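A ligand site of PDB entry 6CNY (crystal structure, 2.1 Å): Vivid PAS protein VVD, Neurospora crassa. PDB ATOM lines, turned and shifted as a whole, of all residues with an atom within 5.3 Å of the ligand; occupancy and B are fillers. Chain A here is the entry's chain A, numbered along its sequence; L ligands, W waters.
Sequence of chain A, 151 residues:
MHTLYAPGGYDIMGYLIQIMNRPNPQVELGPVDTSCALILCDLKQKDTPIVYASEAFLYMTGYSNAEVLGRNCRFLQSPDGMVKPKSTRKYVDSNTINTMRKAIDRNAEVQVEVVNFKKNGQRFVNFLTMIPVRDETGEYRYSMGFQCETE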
ATOM      1  N   ILE A  39      26.129  19.948  12.410  1.00  0.00           N
ATOM      2  CA  ILE A  39      25.449  18.702  12.508  1.00  0.00           C
ATOM      3  C   ILE A  39      24.938  18.330  11.156  1.00  0.00           C
ATOM      4  O   ILE A  39      24.764  19.177  10.272  1.00  0.00           O
ATOM      5  CB  ILE A  39      24.281  18.708  13.490  1.00  0.00           C
ATOM      6  CG1 ILE A  39      23.171  19.654  13.019  1.00  0.00           C
ATOM      7  CG2 ILE A  39      24.747  19.014  14.941  1.00  0.00           C
ATOM      8  CD1 ILE A  39      22.175  19.885  14.119  1.00  0.00           C
ATOM      9  N   LEU A  40      24.739  17.028  10.969  1.00  0.00           N
ATOM     10  CA  LEU A  40      24.095  16.529   9.765  1.00  0.00           C
ATOM     11  C   LEU A  40      22.858  15.810  10.212  1.00  0.00           C
ATOM     12  O   LEU A  40      22.923  15.005  11.162  1.00  0.00           O
ATOM     13  CB  LEU A  40      25.021  15.547   9.080  1.00  0.00           C
ATOM     14  CG  LEU A  40      24.588  15.122   7.680  1.00  0.00           C
ATOM     15  CD1 LEU A  40      24.877  16.232   6.689  1.00  0.00           C
ATOM     16  CD2 LEU A  40      25.277  13.858   7.251  1.00  0.00           C
ATOM     17  N   CYS A  41      21.732  16.088   9.547  1.00  0.00           N
ATOM     18  CA  CYS A  41      20.442  15.459   9.831  1.00  0.00           C
ATOM     19  C   CYS A  41      19.986  14.693   8.624  1.00  0.00           C
ATOM     20  O   CYS A  41      20.274  15.082   7.473  1.00  0.00           O
ATOM     21  CB  CYS A  41      19.423  16.479  10.201  1.00  0.00           C
ATOM     22  SG  CYS A  41      19.767  17.357  11.769  1.00  0.00           S
ATOM     23  N   ASP A  47      11.237  12.522  11.325  1.00  0.00           N
ATOM     24  CA  ASP A  47      11.470  13.742  12.075  1.00  0.00           C
ATOM     25  C   ASP A  47      12.925  14.289  12.014  1.00  0.00           C
ATOM     26  O   ASP A  47      13.393  14.990  12.936  1.00  0.00           O
ATOM     27  CB  ASP A  47      10.996  13.551  13.514  1.00  0.00           C
ATOM     28  CG  ASP A  47      10.735  14.884  14.224  1.00  0.00           C
ATOM     29  OD1 ASP A  47      10.399  15.898  13.566  1.00  0.00           O
ATOM     30  OD2 ASP A  47      10.899  14.923  15.449  1.00  0.00           O
ATOM     31  N   THR A  48      13.593  14.021  10.894  1.00  0.00           N
ATOM     32  CA  THR A  48      14.858  14.635  10.515  1.00  0.00           C
ATOM     33  C   THR A  48      15.910  14.589  11.637  1.00  0.00           C
ATOM     34  O   THR A  48      16.310  15.614  12.168  1.00  0.00           O
ATOM     35  CB  THR A  48      14.609  16.066  10.044  1.00  0.00           C
ATOM     36  OG1 THR A  48      13.487  16.084   9.154  1.00  0.00           O
ATOM     37  CG2 THR A  48      15.809  16.603   9.286  1.00  0.00           C
ATOM     38  N   PHE A  57      30.030  21.327  18.176  1.00  0.00           N
ATOM     39  CA  PHE A  57      28.596  21.406  18.513  1.00  0.00           C
ATOM     40  C   PHE A  57      28.297  20.866  19.912  1.00  0.00           C
ATOM     41  O   PHE A  57      27.551  21.470  20.698  1.00  0.00           O
ATOM     42  CB  PHE A  57      27.761  20.672  17.480  1.00  0.00           C
ATOM     43  CG  PHE A  57      26.300  20.587  17.837  1.00  0.00           C
ATOM     44  CD1 PHE A  57      25.420  21.568  17.430  1.00  0.00           C
ATOM     45  CD2 PHE A  57      25.815  19.495  18.529  1.00  0.00           C
ATOM     46  CE1 PHE A  57      24.062  21.463  17.737  1.00  0.00           C
ATOM     47  CE2 PHE A  57      24.480  19.373  18.834  1.00  0.00           C
ATOM     48  CZ  PHE A  57      23.618  20.359  18.440  1.00  0.00           C
ATOM     49  N   ASN A  72      15.624  15.217  16.694  1.00  0.00           N
ATOM     50  CA  ASN A  72      15.469  16.480  15.985  1.00  0.00           C
ATOM     51  C   ASN A  72      16.107  17.572  16.845  1.00  0.00           C
ATOM     52  O   ASN A  72      15.954  17.602  18.077  1.00  0.00           O
ATOM     53  CB  ASN A  72      13.987  16.814  15.803  1.00  0.00           C
ATOM     54  CG  ASN A  72      13.773  17.992  14.894  1.00  0.00           C
ATOM     55  OD1 ASN A  72      13.869  19.150  15.322  1.00  0.00           O
ATOM     56  ND2 ASN A  72      13.504  17.701  13.621  1.00  0.00           N
ATOM     57  N   CYS A  73      16.818  18.496  16.197  1.00  0.00           N
ATOM     58  CA  CYS A  73      17.545  19.553  16.905  1.00  0.00           C
ATOM     59  C   CYS A  73      16.668  20.579  17.620  1.00  0.00           C
ATOM     60  O   CYS A  73      17.217  21.400  18.345  1.00  0.00           O
ATOM     61  CB  CYS A  73      18.515  20.276  15.962  1.00  0.00           C
ATOM     62  SG  CYS A  73      20.017  20.897  16.765  1.00  0.00           S
ATOM     63  N   ARG A  74      15.340  20.524  17.455  1.00  0.00           N
ATOM     64  CA  ARG A  74      14.446  21.437  18.140  1.00  0.00           C
ATOM     65  C   ARG A  74      14.528  21.391  19.669  1.00  0.00           C
ATOM     66  O   ARG A  74      14.092  22.354  20.311  1.00  0.00           O
ATOM     67  CB  ARG A  74      12.984  21.257  17.697  1.00  0.00           C
ATOM     68  CG  ARG A  74      12.274  20.032  18.252  1.00  0.00           C
ATOM     69  CD  ARG A  74      10.803  20.067  17.980  1.00  0.00           C
ATOM     70  NE  ARG A  74      10.528  19.824  16.560  1.00  0.00           N
ATOM     71  CZ  ARG A  74      10.563  18.626  15.978  1.00  0.00           C
ATOM     72  NH1 ARG A  74      10.296  18.527  14.685  1.00  0.00           N
ATOM     73  NH2 ARG A  74      10.859  17.522  16.669  1.00  0.00           N
ATOM     74  N   LEU A  76      16.987  21.975  21.462  1.00  0.00           N
ATOM     75  CA  LEU A  76      17.739  23.166  21.844  1.00  0.00           C
ATOM     76  C   LEU A  76      16.888  24.417  22.134  1.00  0.00           C
ATOM     77  O   LEU A  76      17.383  25.358  22.740  1.00  0.00           O
ATOM     78  CB  LEU A  76      18.778  23.472  20.763  1.00  0.00           C
ATOM     79  CG  LEU A  76      19.929  22.499  20.563  1.00  0.00           C
ATOM     80  CD1 LEU A  76      20.823  23.027  19.450  1.00  0.00           C
ATOM     81  CD2 LEU A  76      20.722  22.331  21.841  1.00  0.00           C
ATOM     82  N   GLN A  77      15.622  24.410  21.700  1.00  0.00           N
ATOM     83  CA  GLN A  77      14.764  25.576  21.850  1.00  0.00           C
ATOM     84  C   GLN A  77      14.147  25.728  23.242  1.00  0.00           C
ATOM     85  O   GLN A  77      13.511  26.752  23.504  1.00  0.00           O
ATOM     86  CB  GLN A  77      13.705  25.583  20.745  1.00  0.00           C
ATOM     87  CG  GLN A  77      14.318  25.676  19.383  1.00  0.00           C
ATOM     88  CD  GLN A  77      13.434  25.186  18.268  1.00  0.00           C
ATOM     89  OE1 GLN A  77      12.212  24.942  18.432  1.00  0.00           O
ATOM     90  NE2 GLN A  77      14.071  25.042  17.075  1.00  0.00           N
ATOM     91  N   PRO A  85       6.949  18.769  18.421  1.00  0.00           N
ATOM     92  CA  PRO A  85       6.709  19.442  17.137  1.00  0.00           C
ATOM     93  C   PRO A  85       5.302  20.021  17.073  1.00  0.00           C
ATOM     94  O   PRO A  85       4.415  19.509  17.768  1.00  0.00           O
ATOM     95  CB  PRO A  85       6.871  18.309  16.097  1.00  0.00           C
ATOM     96  CG  PRO A  85       6.753  17.026  16.875  1.00  0.00           C
ATOM     97  CD  PRO A  85       7.186  17.328  18.280  1.00  0.00           C
ATOM     98  N   LYS A  86       5.117  21.088  16.296  1.00  0.00           N
ATOM     99  CA  LYS A  86       3.816  21.790  16.215  1.00  0.00           C
ATOM    100  C   LYS A  86       3.392  22.569  17.480  1.00  0.00           C
ATOM    101  O   LYS A  86       2.418  23.303  17.440  1.00  0.00           O
ATOM    102  CB  LYS A  86       2.663  20.821  15.807  1.00  0.00           C
ATOM    103  CG  LYS A  86       2.911  19.980  14.555  1.00  0.00           C
ATOM    104  CD  LYS A  86       2.569  20.795  13.316  1.00  0.00           C
ATOM    105  CE  LYS A  86       3.103  20.162  12.041  1.00  0.00           C
ATOM    106  NZ  LYS A  86       4.553  20.436  11.829  1.00  0.00           N
ATOM    107  N   ARG A  89       6.320  27.584  20.696  1.00  0.00           N
ATOM    108  CA  ARG A  89       7.549  27.769  21.470  1.00  0.00           C
ATOM    109  C   ARG A  89       7.414  28.945  22.412  1.00  0.00           C
ATOM    110  O   ARG A  89       6.917  30.012  22.026  1.00  0.00           O
ATOM    111  CB  ARG A  89       8.750  27.977  20.584  1.00  0.00           C
ATOM    112  CG  ARG A  89       9.513  26.686  20.308  1.00  0.00           C
ATOM    113  CD  ARG A  89       8.671  25.609  19.709  1.00  0.00           C
ATOM    114  NE  ARG A  89       9.488  24.813  18.861  1.00  0.00           N
ATOM    115  CZ  ARG A  89       9.077  24.019  17.865  1.00  0.00           C
ATOM    116  NH1 ARG A  89      10.017  23.431  17.131  1.00  0.00           N
ATOM    117  NH2 ARG A  89       7.828  23.865  17.548  1.00  0.00           N
ATOM    118  N   ILE A  97      10.447  29.639  13.515  1.00  0.00           N
ATOM    119  CA  ILE A  97      10.246  28.192  13.503  1.00  0.00           C
ATOM    120  C   ILE A  97       9.697  27.742  12.150  1.00  0.00           C
ATOM    121  O   ILE A  97      10.155  26.752  11.600  1.00  0.00           O
ATOM    122  CB  ILE A  97       9.265  27.747  14.624  1.00  0.00           C
ATOM    123  CG1 ILE A  97       9.781  28.092  16.034  1.00  0.00           C
ATOM    124  CG2 ILE A  97       8.931  26.281  14.561  1.00  0.00           C
ATOM    125  CD1 ILE A  97      11.014  27.317  16.461  1.00  0.00           C
ATOM    126  N   MET A 100      12.214  27.996   9.270  1.00  0.00           N
ATOM    127  CA  MET A 100      13.123  26.858   9.300  1.00  0.00           C
ATOM    128  C   MET A 100      12.449  25.594   8.739  1.00  0.00           C
ATOM    129  O   MET A 100      13.024  24.925   7.863  1.00  0.00           O
ATOM    130  CB  MET A 100      13.607  26.580  10.722  1.00  0.00           C
ATOM    131  CG  MET A 100      14.570  27.634  11.285  1.00  0.00           C
ATOM    132  SD  MET A 100      15.334  27.048  12.823  1.00  0.00           S
ATOM    133  CE  MET A 100      14.006  27.265  13.959  1.00  0.00           C
ATOM    134  N   ARG A 101      11.244  25.271   9.223  1.00  0.00           N
ATOM    135  CA  ARG A 101      10.606  24.052   8.794  1.00  0.00           C
ATOM    136  C   ARG A 101      10.348  24.037   7.278  1.00  0.00           C
ATOM    137  O   ARG A 101      10.572  23.017   6.599  1.00  0.00           O
ATOM    138  CB  ARG A 101       9.261  23.809   9.517  1.00  0.00           C
ATOM    139  CG  ARG A 101       8.791  22.339   9.337  1.00  0.00           C
ATOM    140  CD  ARG A 101       7.444  22.050   9.913  1.00  0.00           C
ATOM    141  NE  ARG A 101       6.550  23.123   9.505  1.00  0.00           N
ATOM    142  CZ  ARG A 101       6.169  24.175  10.232  1.00  0.00           C
ATOM    143  NH1 ARG A 101       6.586  24.380  11.499  1.00  0.00           N
ATOM    144  NH2 ARG A 101       5.415  25.072   9.617  1.00  0.00           N
ATOM    145  N   ILE A 104      13.594  23.667   5.221  1.00  0.00           N
ATOM    146  CA  ILE A 104      14.059  22.298   5.261  1.00  0.00           C
ATOM    147  C   ILE A 104      13.202  21.387   4.365  1.00  0.00           C
ATOM    148  O   ILE A 104      13.751  20.562   3.631  1.00  0.00           O
ATOM    149  CB  ILE A 104      14.134  21.753   6.696  1.00  0.00           C
ATOM    150  CG1 ILE A 104      15.184  22.540   7.529  1.00  0.00           C
ATOM    151  CG2 ILE A 104      14.498  20.279   6.699  1.00  0.00           C
ATOM    152  CD1 ILE A 104      14.917  22.471   9.021  1.00  0.00           C
ATOM    153  N   VAL A 114      18.279  32.246  16.419  1.00  0.00           N
ATOM    154  CA  VAL A 114      17.323  31.605  17.305  1.00  0.00           C
ATOM    155  C   VAL A 114      17.884  31.515  18.691  1.00  0.00           C
ATOM    156  O   VAL A 114      19.081  31.244  18.860  1.00  0.00           O
ATOM    157  CB  VAL A 114      16.941  30.175  16.760  1.00  0.00           C
ATOM    158  CG1 VAL A 114      18.088  29.187  16.811  1.00  0.00           C
ATOM    159  CG2 VAL A 114      15.744  29.629  17.437  1.00  0.00           C
ATOM    160  N   VAL A 115      17.035  31.743  19.694  1.00  0.00           N
ATOM    161  CA  VAL A 115      17.414  31.508  21.088  1.00  0.00           C
ATOM    162  C   VAL A 115      17.406  30.022  21.337  1.00  0.00           C
ATOM    163  O   VAL A 115      16.415  29.321  21.057  1.00  0.00           O
ATOM    164  CB  VAL A 115      16.492  32.252  22.083  1.00  0.00           C
ATOM    165  CG1 VAL A 115      16.772  31.906  23.504  1.00  0.00           C
ATOM    166  CG2 VAL A 115      16.681  33.739  21.919  1.00  0.00           C
ATOM    167  N   ASN A 116      18.521  29.548  21.876  1.00  0.00           N
ATOM    168  CA  ASN A 116      18.686  28.132  22.194  1.00  0.00           C
ATOM    169  C   ASN A 116      19.209  28.048  23.623  1.00  0.00           C
ATOM    170  O   ASN A 116      19.621  29.084  24.195  1.00  0.00           O
ATOM    171  CB  ASN A 116      19.702  27.479  21.227  1.00  0.00           C
ATOM    172  CG  ASN A 116      19.115  26.998  19.895  1.00  0.00           C
ATOM    173  OD1 ASN A 116      19.862  26.511  19.032  1.00  0.00           O
ATOM    174  ND2 ASN A 116      17.844  27.102  19.717  1.00  0.00           N
ATOM    175  N   ASN A 126      21.846  31.641  18.755  1.00  0.00           N
ATOM    176  CA  ASN A 126      22.425  30.706  17.800  1.00  0.00           C
ATOM    177  C   ASN A 126      22.201  31.289  16.434  1.00  0.00           C
ATOM    178  O   ASN A 126      21.028  31.413  15.979  1.00  0.00           O
ATOM    179  CB  ASN A 126      21.754  29.343  17.967  1.00  0.00           C
ATOM    180  CG  ASN A 126      22.367  28.263  17.080  1.00  0.00           C
ATOM    181  OD1 ASN A 126      23.158  28.519  16.141  1.00  0.00           O
ATOM    182  ND2 ASN A 126      21.968  26.990  17.390  1.00  0.00           N
ATOM    183  N   LEU A 128      22.242  30.401  12.924  1.00  0.00           N
ATOM    184  CA  LEU A 128      22.079  29.064  12.387  1.00  0.00           C
ATOM    185  C   LEU A 128      21.904  29.109  10.862  1.00  0.00           C
ATOM    186  O   LEU A 128      21.039  29.841  10.356  1.00  0.00           O
ATOM    187  CB  LEU A 128      20.850  28.425  13.037  1.00  0.00           C
ATOM    188  CG  LEU A 128      20.337  27.079  12.523  1.00  0.00           C
ATOM    189  CD1 LEU A 128      21.442  26.023  12.664  1.00  0.00           C
ATOM    190  CD2 LEU A 128      19.091  26.751  13.364  1.00  0.00           C
ATOM    191  N   MET A 130      21.343  26.434   7.527  1.00  0.00           N
ATOM    192  CA  MET A 130      21.038  25.074   7.146  1.00  0.00           C
ATOM    193  C   MET A 130      21.094  24.999   5.647  1.00  0.00           C
ATOM    194  O   MET A 130      20.469  25.803   4.960  1.00  0.00           O
ATOM    195  CB  MET A 130      19.671  24.637   7.677  1.00  0.00           C
ATOM    196  CG  MET A 130      19.668  24.666   9.216  1.00  0.00           C
ATOM    197  SD  MET A 130      18.100  24.570  10.034  1.00  0.00           S
ATOM    198  CE  MET A 130      17.159  25.874   9.403  1.00  0.00           C
ATOM    199  N   SER A 143      20.656  17.352   5.590  1.00  0.00           N
ATOM    200  CA  SER A 143      20.761  18.805   5.770  1.00  0.00           C
ATOM    201  C   SER A 143      21.917  18.993   6.686  1.00  0.00           C
ATOM    202  O   SER A 143      22.013  18.305   7.719  1.00  0.00           O
ATOM    203  CB  SER A 143      19.506  19.401   6.405  1.00  0.00           C
ATOM    204  OG  SER A 143      19.643  20.826   6.534  1.00  0.00           O
ATOM    205  N   MET A 144      22.797  19.919   6.348  1.00  0.00           N
ATOM    206  CA  MET A 144      23.901  20.232   7.207  1.00  0.00           C
ATOM    207  C   MET A 144      23.619  21.592   7.825  1.00  0.00           C
ATOM    208  O   MET A 144      23.279  22.542   7.117  1.00  0.00           O
ATOM    209  CB  MET A 144      25.207  20.229   6.467  1.00  0.00           C
ATOM    210  CG  MET A 144      26.409  20.318   7.464  1.00  0.00           C
ATOM    211  SD  MET A 144      27.998  20.123   6.680  1.00  0.00           S
ATOM    212  CE  MET A 144      28.107  18.367   6.499  1.00  0.00           C
ATOM    213  N   GLY A 145      23.706  21.634   9.149  1.00  0.00           N
ATOM    214  CA  GLY A 145      23.455  22.825   9.953  1.00  0.00           C
ATOM    215  C   GLY A 145      24.734  23.335  10.584  1.00  0.00           C
ATOM    216  O   GLY A 145      25.552  22.547  11.053  1.00  0.00           O
ATOM    217  N   GLN A 147      26.171  26.088  13.366  1.00  0.00           N
ATOM    218  CA  GLN A 147      25.722  26.869  14.522  1.00  0.00           C
ATOM    219  C   GLN A 147      26.856  27.786  14.979  1.00  0.00           C
ATOM    220  O   GLN A 147      27.987  27.351  15.015  1.00  0.00           O
ATOM    221  CB  GLN A 147      25.370  25.933  15.672  1.00  0.00           C
ATOM    222  CG  GLN A 147      24.120  25.113  15.475  1.00  0.00           C
ATOM    223  CD  GLN A 147      24.335  23.793  14.712  1.00  0.00           C
ATOM    224  OE1 GLN A 147      25.473  23.344  14.503  1.00  0.00           O
ATOM    225  NE2 GLN A 147      23.226  23.180  14.299  1.00  0.00           N
HETATM  226  N1  LIG L   1      16.979  24.291  15.525  1.00  0.00           N
HETATM  227  C1  LIG L   1      17.525  24.976  16.558  1.00  0.00           C
HETATM  228  O1  LIG L   1      16.814  25.659  17.304  1.00  0.00           O
HETATM  229  N2  LIG L   1      18.899  24.990  16.740  1.00  0.00           N
HETATM  230  C2  LIG L   1      19.837  24.346  15.945  1.00  0.00           C
HETATM  231  O2  LIG L   1      21.043  24.439  16.204  1.00  0.00           O
HETATM  232  C3  LIG L   1      19.248  23.633  14.816  1.00  0.00           C
HETATM  233  N3  LIG L   1      20.050  23.044  13.975  1.00  0.00           N
HETATM  234  C4  LIG L   1      19.469  22.356  12.905  1.00  0.00           C
HETATM  235  C5  LIG L   1      20.299  21.747  11.968  1.00  0.00           C
HETATM  236  C6  LIG L   1      19.781  21.063  10.877  1.00  0.00           C
HETATM  237  C7  LIG L   1      20.709  20.522   9.820  1.00  0.00           C
HETATM  238  C8  LIG L   1      18.387  20.951  10.733  1.00  0.00           C
HETATM  239  C9  LIG L   1      17.782  20.145   9.611  1.00  0.00           C
HETATM  240  C10 LIG L   1      17.548  21.566  11.656  1.00  0.00           C
HETATM  241  C11 LIG L   1      18.072  22.288  12.730  1.00  0.00           C
HETATM  242  N4  LIG L   1      17.253  22.992  13.627  1.00  0.00           N
HETATM  243  C12 LIG L   1      17.796  23.664  14.694  1.00  0.00           C
HETATM  244  C13 LIG L   1      15.823  23.226  13.341  1.00  0.00           C
HETATM  245  C14 LIG L   1      14.881  22.249  14.021  1.00  0.00           C
HETATM  246  O3  LIG L   1      15.412  20.929  13.969  1.00  0.00           O
HETATM  247  C15 LIG L   1      13.507  22.234  13.352  1.00  0.00           C
HETATM  248  O4  LIG L   1      13.665  22.011  11.954  1.00  0.00           O
HETATM  249  C16 LIG L   1      12.714  23.531  13.538  1.00  0.00           C
HETATM  250  O5  LIG L   1      12.257  23.622  14.889  1.00  0.00           O
HETATM  251  C17 LIG L   1      11.545  23.651  12.576  1.00  0.00           C
HETATM  252  O6  LIG L   1      10.846  22.386  12.467  1.00  0.00           O
HETATM  253  P1  LIG L   1       9.629  22.087  13.504  1.00  0.00           P
HETATM  254  O7  LIG L   1       8.569  23.087  13.187  1.00  0.00           O
HETATM  255  O8  LIG L   1       9.355  20.676  13.244  1.00  0.00           O
HETATM  256  O9  LIG L   1      10.165  22.228  14.868  1.00  0.00           O
HETATM  257  O   HOH W   1       6.768  23.604  15.202  1.00  0.00           O
HETATM  258  O   HOH W   2      11.826  20.281  10.846  1.00  0.00           O
HETATM  259  O   HOH W   3      16.927  18.391  13.168  1.00  0.00           O
HETATM  260  O   HOH W   4      14.246  19.488  11.292  1.00  0.00           O
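OE1 of Gln 77 is in hydrogen-bond range of NE of Arg 89, at 2.8 Å. The side-chain amide oxygen of Asn 72 is in hydrogen-bond range of the backbone NH of Arg 74 (2.9 Å). ND2 of Asn 126 lies within hydrogen-bond range of OD1 of Asn 116, at 2.7 Å. NH1 of Arg 74 lies within salt-bridge range of OD1 of Asp 47, 2.9 Å away. N of Gly 145 sits at hydrogen-bond distance from O of Ile 39, at 2.9 Å. The backbone carbonyl oxygen (O) of Ser 143 lies within hydrogen-bond range of the backbone NH (N) of Cys 41 (2.9 Å). N of Asn 126 lies within hydrogen-bond range of O of Val 114 (2.8 Å). ND2 of Asn 72 is in hydrogen-bond range of O of Asp 47 (2.8 Å).
O1 of the ligand lies within hydrogen-bond range of NE2 of Gln 77, 2.8 Å away. The side-chain amide oxygen (OD1) of Asn 116 is in hydrogen-bond range of a nitrogen (N2) of the ligand, at 2.9 Å. NH1 of Arg 74 is in salt-bridge range of O8 of the ligand (2.8 Å). The side-chain amide oxygen of Asn 72 lies within hydrogen-bond range of an oxygen (O3) of the ligand (2.7 Å). ND2 of Asn 126 lies within hydrogen-bond range of O2 of the ligand (3.0 Å). O9 of the ligand is in salt-bridge range of NH1 of Arg 89, at 2.6 Å. The side-chain sulfur of Cys 73 sits close to a nitrogen (N3) of the ligand. The side-chain amide nitrogen (NE2) of Gln 147 lies within hydrogen-bond range of an oxygen (O2) of the ligand (3.2 Å). The guanidinium group (NH1) of Arg 101 lies within salt-bridge range of an oxygen (O7) of the ligand.
Merely in contact with the ligand: Ile 104 (3.2 Å), Gly 145 (3.3 Å), Ser 143 (3.3 Å), Ile 39 (3.4 Å), Leu 128 (3.4 Å), Met 130 (3.5 Å), Ile 97 (3.5 Å), Leu 76 (3.5 Å), Met 144 (3.7 Å), Val 114 (3.8 Å), Cys 41 (3.8 Å) and Met 100 (3.9 Å). Hydrophobic or aromatic side chains that line the ligand: Ile 39, Leu 76, Ile 97, Met 100, Ile 104, Val 114, Leu 128 and Met 130. Of the 28 residues printed, 21 come within 4 Å of the ligand.
Water W4 lies within hydrogen-bond range of an oxygen (O4) of the ligand (2.7 Å) and the side-chain amide nitrogen (ND2) of Asn 72 (3.0 Å). Water W1 lies within hydrogen-bond range of NH2 of Arg 89 (2.6 Å), O7 of the ligand (2.8 Å) and N of Lys 86 (3.2 Å). Water W3 lies within hydrogen-bond range of O of Thr 48 (3.0 Å), N of Cys 73 (3.0 Å), O3 of the ligand (3.1 Å) and SG of Cys 41 (3.3 Å).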
